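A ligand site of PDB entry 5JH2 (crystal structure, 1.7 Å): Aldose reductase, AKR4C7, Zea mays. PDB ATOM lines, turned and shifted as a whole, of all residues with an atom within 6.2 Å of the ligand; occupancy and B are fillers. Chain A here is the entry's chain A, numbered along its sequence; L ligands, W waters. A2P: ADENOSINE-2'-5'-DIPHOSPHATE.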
ATOM      1  N   HIS A 180      25.976  13.628  -8.611  1.00  0.00           N
ATOM      2  CA  HIS A 180      25.840  14.728  -9.572  1.00  0.00           C
ATOM      3  C   HIS A 180      27.052  15.667  -9.474  1.00  0.00           C
ATOM      4  O   HIS A 180      27.916  15.448  -8.650  1.00  0.00           O
ATOM      5  CB  HIS A 180      24.484  15.443  -9.391  1.00  0.00           C
ATOM      6  CG  HIS A 180      24.314  16.045  -8.040  1.00  0.00           C
ATOM      7  ND1 HIS A 180      24.913  17.217  -7.684  1.00  0.00           N
ATOM      8  CD2 HIS A 180      23.635  15.637  -6.943  1.00  0.00           C
ATOM      9  CE1 HIS A 180      24.592  17.540  -6.440  1.00  0.00           C
ATOM     10  NE2 HIS A 180      23.833  16.582  -5.969  1.00  0.00           N
ATOM     11  N   TYR A 202      21.224   8.546  -8.748  1.00  0.00           N
ATOM     12  CA  TYR A 202      19.933   9.231  -8.577  1.00  0.00           C
ATOM     13  C   TYR A 202      20.160  10.686  -8.324  1.00  0.00           C
ATOM     14  O   TYR A 202      21.276  11.121  -8.024  1.00  0.00           O
ATOM     15  CB  TYR A 202      19.000   8.522  -7.546  1.00  0.00           C
ATOM     16  CG  TYR A 202      19.314   8.659  -6.098  1.00  0.00           C
ATOM     17  CD1 TYR A 202      19.071   9.875  -5.406  1.00  0.00           C
ATOM     18  CD2 TYR A 202      19.758   7.572  -5.380  1.00  0.00           C
ATOM     19  CE1 TYR A 202      19.327   9.982  -4.048  1.00  0.00           C
ATOM     20  CE2 TYR A 202      20.024   7.669  -4.003  1.00  0.00           C
ATOM     21  CZ  TYR A 202      19.786   8.868  -3.351  1.00  0.00           C
ATOM     22  OH  TYR A 202      20.052   8.913  -2.007  1.00  0.00           O
ATOM     23  N   SER A 203      19.075  11.454  -8.469  1.00  0.00           N
ATOM     24  CA  SER A 203      19.163  12.917  -8.465  1.00  0.00           C
ATOM     25  C   SER A 203      20.357  13.435  -9.252  1.00  0.00           C
ATOM     26  O   SER A 203      21.136  14.187  -8.727  1.00  0.00           O
ATOM     27  CB  SER A 203      19.212  13.475  -6.995  1.00  0.00           C
ATOM     28  OG  SER A 203      18.006  13.094  -6.347  1.00  0.00           O
ATOM     29  N   PRO A 204      20.450  13.099 -10.552  1.00  0.00           N
ATOM     30  CA  PRO A 204      21.711  13.398 -11.318  1.00  0.00           C
ATOM     31  C   PRO A 204      21.736  14.878 -11.752  1.00  0.00           C
ATOM     32  O   PRO A 204      22.731  15.349 -12.208  1.00  0.00           O
ATOM     33  CB  PRO A 204      21.584  12.509 -12.536  1.00  0.00           C
ATOM     34  CG  PRO A 204      20.117  12.377 -12.725  1.00  0.00           C
ATOM     35  CD  PRO A 204      19.520  12.294 -11.363  1.00  0.00           C
ATOM     36  N   LEU A 205      20.623  15.592 -11.542  1.00  0.00           N
ATOM     37  CA  LEU A 205      20.574  17.055 -11.694  1.00  0.00           C
ATOM     38  C   LEU A 205      20.638  17.851 -10.354  1.00  0.00           C
ATOM     39  O   LEU A 205      20.468  19.096 -10.350  1.00  0.00           O
ATOM     40  CB  LEU A 205      19.327  17.417 -12.539  1.00  0.00           C
ATOM     41  CG  LEU A 205      19.141  16.675 -13.850  1.00  0.00           C
ATOM     42  CD1 LEU A 205      17.930  17.178 -14.626  1.00  0.00           C
ATOM     43  CD2 LEU A 205      20.412  16.744 -14.698  1.00  0.00           C
ATOM     44  N   GLY A 206      20.907  17.159  -9.244  1.00  0.00           N
ATOM     45  CA  GLY A 206      21.055  17.786  -7.904  1.00  0.00           C
ATOM     46  C   GLY A 206      19.736  18.003  -7.168  1.00  0.00           C
ATOM     47  O   GLY A 206      18.764  17.348  -7.553  1.00  0.00           O
ATOM     48  N   LEU A 218      22.608  23.060 -11.876  1.00  0.00           N
ATOM     49  CA  LEU A 218      22.420  23.559 -13.245  1.00  0.00           C
ATOM     50  C   LEU A 218      22.759  25.038 -13.389  1.00  0.00           C
ATOM     51  O   LEU A 218      22.997  25.479 -14.509  1.00  0.00           O
ATOM     52  CB  LEU A 218      20.983  23.311 -13.750  1.00  0.00           C
ATOM     53  CG  LEU A 218      20.565  21.808 -13.727  1.00  0.00           C
ATOM     54  CD1 LEU A 218      19.276  21.640 -14.464  1.00  0.00           C
ATOM     55  CD2 LEU A 218      21.647  20.920 -14.300  1.00  0.00           C
ATOM     56  N   THR A 233      22.279  21.813 -23.387  1.00  0.00           N
ATOM     57  CA  THR A 233      21.768  22.406 -22.159  1.00  0.00           C
ATOM     58  C   THR A 233      22.591  22.038 -20.931  1.00  0.00           C
ATOM     59  O   THR A 233      23.388  21.100 -20.994  1.00  0.00           O
ATOM     60  CB  THR A 233      20.324  21.958 -21.913  1.00  0.00           C
ATOM     61  OG1 THR A 233      20.320  20.561 -21.552  1.00  0.00           O
ATOM     62  CG2 THR A 233      19.469  22.252 -23.161  1.00  0.00           C
ATOM     63  N   ALA A 235      21.444  20.663 -18.191  1.00  0.00           N
ATOM     64  CA  ALA A 235      21.091  19.300 -17.817  1.00  0.00           C
ATOM     65  C   ALA A 235      21.795  18.265 -18.668  1.00  0.00           C
ATOM     66  O   ALA A 235      22.245  17.250 -18.126  1.00  0.00           O
ATOM     67  CB  ALA A 235      19.606  19.103 -17.892  1.00  0.00           C
ATOM     68  N   GLN A 236      21.878  18.485 -19.980  1.00  0.00           N
ATOM     69  CA  GLN A 236      22.511  17.518 -20.859  1.00  0.00           C
ATOM     70  C   GLN A 236      23.929  17.303 -20.446  1.00  0.00           C
ATOM     71  O   GLN A 236      24.410  16.216 -20.462  1.00  0.00           O
ATOM     72  CB  GLN A 236      22.492  17.950 -22.326  1.00  0.00           C
ATOM     73  CG  GLN A 236      21.194  17.676 -23.095  1.00  0.00           C
ATOM     74  CD  GLN A 236      21.272  18.256 -24.509  1.00  0.00           C
ATOM     75  OE1 GLN A 236      21.356  19.483 -24.677  1.00  0.00           O
ATOM     76  NE2 GLN A 236      21.277  17.384 -25.533  1.00  0.00           N
ATOM     77  N   LEU A 239      24.192  15.321 -17.161  1.00  0.00           N
ATOM     78  CA  LEU A 239      23.892  13.915 -17.396  1.00  0.00           C
ATOM     79  C   LEU A 239      25.044  13.229 -18.091  1.00  0.00           C
ATOM     80  O   LEU A 239      25.541  12.156 -17.668  1.00  0.00           O
ATOM     81  CB  LEU A 239      22.620  13.803 -18.197  1.00  0.00           C
ATOM     82  CG  LEU A 239      21.395  14.205 -17.393  1.00  0.00           C
ATOM     83  CD1 LEU A 239      20.213  14.310 -18.361  1.00  0.00           C
ATOM     84  CD2 LEU A 239      21.108  13.264 -16.209  1.00  0.00           C
ATOM     85  N   LEU A 250      19.496   8.627 -13.491  1.00  0.00           N
ATOM     86  CA  LEU A 250      18.030   8.554 -13.321  1.00  0.00           C
ATOM     87  C   LEU A 250      17.351   9.915 -13.298  1.00  0.00           C
ATOM     88  O   LEU A 250      16.712  10.275 -12.352  1.00  0.00           O
ATOM     89  CB  LEU A 250      17.739   7.764 -12.075  1.00  0.00           C
ATOM     90  CG  LEU A 250      18.140   6.270 -12.161  1.00  0.00           C
ATOM     91  CD1 LEU A 250      17.874   5.666 -10.795  1.00  0.00           C
ATOM     92  CD2 LEU A 250      17.470   5.517 -13.342  1.00  0.00           C
ATOM     93  N   PRO A 251      17.471  10.690 -14.404  1.00  0.00           N
ATOM     94  CA  PRO A 251      16.785  11.991 -14.341  1.00  0.00           C
ATOM     95  C   PRO A 251      15.243  11.834 -14.197  1.00  0.00           C
ATOM     96  O   PRO A 251      14.678  10.913 -14.751  1.00  0.00           O
ATOM     97  CB  PRO A 251      17.181  12.647 -15.703  1.00  0.00           C
ATOM     98  CG  PRO A 251      17.432  11.521 -16.617  1.00  0.00           C
ATOM     99  CD  PRO A 251      18.009  10.407 -15.733  1.00  0.00           C
ATOM    100  N   LYS A 252      14.595  12.734 -13.442  1.00  0.00           N
ATOM    101  CA  LYS A 252      13.139  12.720 -13.258  1.00  0.00           C
ATOM    102  C   LYS A 252      12.581  14.023 -13.892  1.00  0.00           C
ATOM    103  O   LYS A 252      13.172  15.109 -13.669  1.00  0.00           O
ATOM    104  CB  LYS A 252      12.860  12.812 -11.739  1.00  0.00           C
ATOM    105  CG  LYS A 252      13.282  11.585 -10.993  1.00  0.00           C
ATOM    106  CD  LYS A 252      12.882  11.572  -9.564  1.00  0.00           C
ATOM    107  CE  LYS A 252      13.538  12.615  -8.709  1.00  0.00           C
ATOM    108  NZ  LYS A 252      15.006  12.392  -8.589  1.00  0.00           N
ATOM    109  N   SER A 253      11.473  13.912 -14.632  1.00  0.00           N
ATOM    110  CA  SER A 253      10.807  15.100 -15.208  1.00  0.00           C
ATOM    111  C   SER A 253       9.330  14.735 -15.437  1.00  0.00           C
ATOM    112  O   SER A 253       9.008  13.583 -15.776  1.00  0.00           O
ATOM    113  CB  SER A 253      11.446  15.557 -16.513  1.00  0.00           C
ATOM    114  OG  SER A 253      10.854  16.745 -17.011  1.00  0.00           O
ATOM    115  N   THR A 254       8.463  15.717 -15.240  1.00  0.00           N
ATOM    116  CA  THR A 254       7.069  15.596 -15.702  1.00  0.00           C
ATOM    117  C   THR A 254       6.855  16.357 -17.030  1.00  0.00           C
ATOM    118  O   THR A 254       5.745  16.371 -17.569  1.00  0.00           O
ATOM    119  CB  THR A 254       6.092  16.156 -14.643  1.00  0.00           C
ATOM    120  OG1 THR A 254       6.452  17.478 -14.309  1.00  0.00           O
ATOM    121  CG2 THR A 254       6.170  15.378 -13.347  1.00  0.00           C
ATOM    122  N   ASN A 255       7.905  16.991 -17.559  1.00  0.00           N
ATOM    123  CA  ASN A 255       7.809  17.714 -18.791  1.00  0.00           C
ATOM    124  C   ASN A 255       8.186  16.841 -19.922  1.00  0.00           C
ATOM    125  O   ASN A 255       9.322  16.363 -19.970  1.00  0.00           O
ATOM    126  CB  ASN A 255       8.734  18.954 -18.743  1.00  0.00           C
ATOM    127  CG  ASN A 255       8.665  19.772 -19.978  1.00  0.00           C
ATOM    128  OD1 ASN A 255       9.261  19.476 -21.008  1.00  0.00           O
ATOM    129  ND2 ASN A 255       7.841  20.795 -19.925  1.00  0.00           N
ATOM    130  N   ARG A 258      11.552  17.940 -21.675  1.00  0.00           N
ATOM    131  CA  ARG A 258      12.739  17.651 -20.846  1.00  0.00           C
ATOM    132  C   ARG A 258      12.941  16.145 -20.739  1.00  0.00           C
ATOM    133  O   ARG A 258      14.072  15.681 -20.739  1.00  0.00           O
ATOM    134  CB  ARG A 258      12.626  18.225 -19.451  1.00  0.00           C
ATOM    135  CG  ARG A 258      12.767  19.771 -19.487  1.00  0.00           C
ATOM    136  CD  ARG A 258      12.911  20.359 -18.077  1.00  0.00           C
ATOM    137  NE  ARG A 258      11.671  20.691 -17.389  1.00  0.00           N
ATOM    138  CZ  ARG A 258      10.994  21.847 -17.536  1.00  0.00           C
ATOM    139  NH1 ARG A 258       9.896  22.058 -16.828  1.00  0.00           N
ATOM    140  NH2 ARG A 258      11.406  22.804 -18.386  1.00  0.00           N
ATOM    141  N   ILE A 259      11.834  15.386 -20.706  1.00  0.00           N
ATOM    142  CA  ILE A 259      11.960  13.889 -20.824  1.00  0.00           C
ATOM    143  C   ILE A 259      12.777  13.500 -22.067  1.00  0.00           C
ATOM    144  O   ILE A 259      13.781  12.730 -21.937  1.00  0.00           O
ATOM    145  CB  ILE A 259      10.615  13.144 -20.696  1.00  0.00           C
ATOM    146  CG1 ILE A 259      10.107  13.282 -19.296  1.00  0.00           C
ATOM    147  CG2 ILE A 259      10.756  11.666 -21.054  1.00  0.00           C
ATOM    148  CD1 ILE A 259       8.671  12.816 -19.036  1.00  0.00           C
ATOM    149  N   GLN A 261      14.812  15.469 -23.921  1.00  0.00           N
ATOM    150  CA  GLN A 261      16.184  16.030 -23.853  1.00  0.00           C
ATOM    151  C   GLN A 261      17.097  15.228 -22.940  1.00  0.00           C
ATOM    152  O   GLN A 261      18.330  15.132 -23.186  1.00  0.00           O
ATOM    153  CB  GLN A 261      16.162  17.463 -23.358  1.00  0.00           C
ATOM    154  CG  GLN A 261      15.553  18.406 -24.345  1.00  0.00           C
ATOM    155  CD  GLN A 261      15.472  19.831 -23.779  1.00  0.00           C
ATOM    156  OE1 GLN A 261      15.959  20.103 -22.681  1.00  0.00           O
ATOM    157  NE2 GLN A 261      14.770  20.711 -24.493  1.00  0.00           N
ATOM    158  N   ASN A 262      16.520  14.653 -21.907  1.00  0.00           N
ATOM    159  CA  ASN A 262      17.279  13.876 -20.881  1.00  0.00           C
ATOM    160  C   ASN A 262      17.783  12.558 -21.464  1.00  0.00           C
ATOM    161  O   ASN A 262      18.731  11.979 -20.923  1.00  0.00           O
ATOM    162  CB  ASN A 262      16.508  13.670 -19.597  1.00  0.00           C
ATOM    163  CG  ASN A 262      16.345  14.927 -18.800  1.00  0.00           C
ATOM    164  OD1 ASN A 262      16.982  15.960 -19.082  1.00  0.00           O
ATOM    165  ND2 ASN A 262      15.450  14.897 -17.837  1.00  0.00           N
HETATM  166  P1  A2P L   1      10.630  19.086 -14.296  1.00  0.00           P
HETATM  167  O1P A2P L   1      11.278  18.736 -15.615  1.00  0.00           O
HETATM  168  O2P A2P L   1       9.813  17.953 -13.747  1.00  0.00           O
HETATM  169  O3P A2P L   1       9.815  20.393 -14.429  1.00  0.00           O
HETATM  170  P2  A2P L   1      16.706  15.349  -9.848  1.00  0.00           P
HETATM  171  O4P A2P L   1      18.224  15.760  -9.825  1.00  0.00           O
HETATM  172  O5P A2P L   1      16.143  15.210  -8.443  1.00  0.00           O
HETATM  173  O6P A2P L   1      16.476  14.286 -10.892  1.00  0.00           O
HETATM  174  O5' A2P L   1      16.068  16.726 -10.519  1.00  0.00           O
HETATM  175  C5' A2P L   1      14.656  16.752 -10.717  1.00  0.00           C
HETATM  176  C4' A2P L   1      14.317  18.209 -11.021  1.00  0.00           C
HETATM  177  O4' A2P L   1      14.995  18.509 -12.227  1.00  0.00           O
HETATM  178  C3' A2P L   1      12.830  18.406 -11.282  1.00  0.00           C
HETATM  179  O3' A2P L   1      12.397  19.584 -10.602  1.00  0.00           O
HETATM  180  C2' A2P L   1      12.672  18.551 -12.762  1.00  0.00           C
HETATM  181  O2' A2P L   1      11.648  19.498 -13.156  1.00  0.00           O
HETATM  182  C1' A2P L   1      14.074  19.030 -13.201  1.00  0.00           C
HETATM  183  N9  A2P L   1      14.523  18.642 -14.553  1.00  0.00           N
HETATM  184  C8  A2P L   1      14.428  17.439 -15.132  1.00  0.00           C
HETATM  185  N7  A2P L   1      14.958  17.455 -16.328  1.00  0.00           N
HETATM  186  C5  A2P L   1      15.461  18.707 -16.526  1.00  0.00           C
HETATM  187  C6  A2P L   1      16.124  19.387 -17.610  1.00  0.00           C
HETATM  188  N6  A2P L   1      16.389  18.702 -18.722  1.00  0.00           N
HETATM  189  N1  A2P L   1      16.481  20.731 -17.463  1.00  0.00           N
HETATM  190  C2  A2P L   1      16.133  21.345 -16.329  1.00  0.00           C
HETATM  191  N3  A2P L   1      15.502  20.800 -15.264  1.00  0.00           N
HETATM  192  C4  A2P L   1      15.139  19.471 -15.341  1.00  0.00           C
HETATM  193  O   HOH W   1      18.889  22.274 -18.495  1.00  0.00           O
HETATM  194  O   HOH W   2      17.998  19.466 -21.058  1.00  0.00           O
HETATM  195  O   HOH W   3       7.073  19.770 -15.139  1.00  0.00           O
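O of Ser 203 sits close to O4P of the ligand, at 3.5 Å. N of Pro 204 touches O4P of the ligand (3.5 Å). CD1 of Leu 218 touches C2 of the ligand, at 3.7 Å. Ala 235 touches the ligand (CB to N6, 3.3 Å). Within 4 Å of the ligand: Ser 203, Pro 204, Leu 205, Gly 206, Leu 218, Ala 235, Lys 252, Ser 253, Thr 254, Arg 258 and Asn 262. The nearest printed residue that does not touch the ligand is Asn 255 (4.04 Å).
Water W3 bridges the side-chain hydroxyl of Thr 254 (2.5 Å) and an oxygen (O3P) of the ligand (2.9 Å). Water W2 lies within hydrogen-bond range of the side-chain hydroxyl (OG1) of Thr 233 (2.6 Å), the side-chain amide oxygen (OE1) of Gln 261 (2.7 Å) and a nitrogen (N6) of the ligand (2.9 Å). Water W1 lies within hydrogen-bond range of N of Ala 235 and N1 of the ligand.
OG of Ser 253 is in hydrogen-bond range of O1P of the ligand, 2.5 Å away. NE of Arg 258 is in salt-bridge range of O1P of the ligand. O4P of the ligand lies within hydrogen-bond range of N of Gly 206. The backbone carbonyl oxygen of Gly 206 sits close to an oxygen (O4P) of the ligand (2.8 Å). A nitrogen (N6) of the ligand lies within hydrogen-bond range of the side-chain amide oxygen (OD1) of Asn 262. O4P of the ligand is in hydrogen-bond range of N of Leu 205 (3.0 Å). The backbone NH (N) of Thr 254 sits at hydrogen-bond distance from an oxygen (O2P) of the ligand. The side-chain hydroxyl of Thr 254 is in hydrogen-bond range of an oxygen (O2P) of the ligand (3.4 Å). NZ of Lys 252 lies within salt-bridge range of O5P of the ligand (3.0 Å).
The backbone NH (N) of Asn 255 is in hydrogen-bond range of the side-chain hydroxyl (OG) of Ser 253, 3.0 Å away. The backbone carbonyl oxygen of Arg 258 lies close to the side-chain amide nitrogen of Asn 262 (3.3 Å). OD1 of Asn 255 sits at hydrogen-bond distance from N of Arg 258 (2.8 Å).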
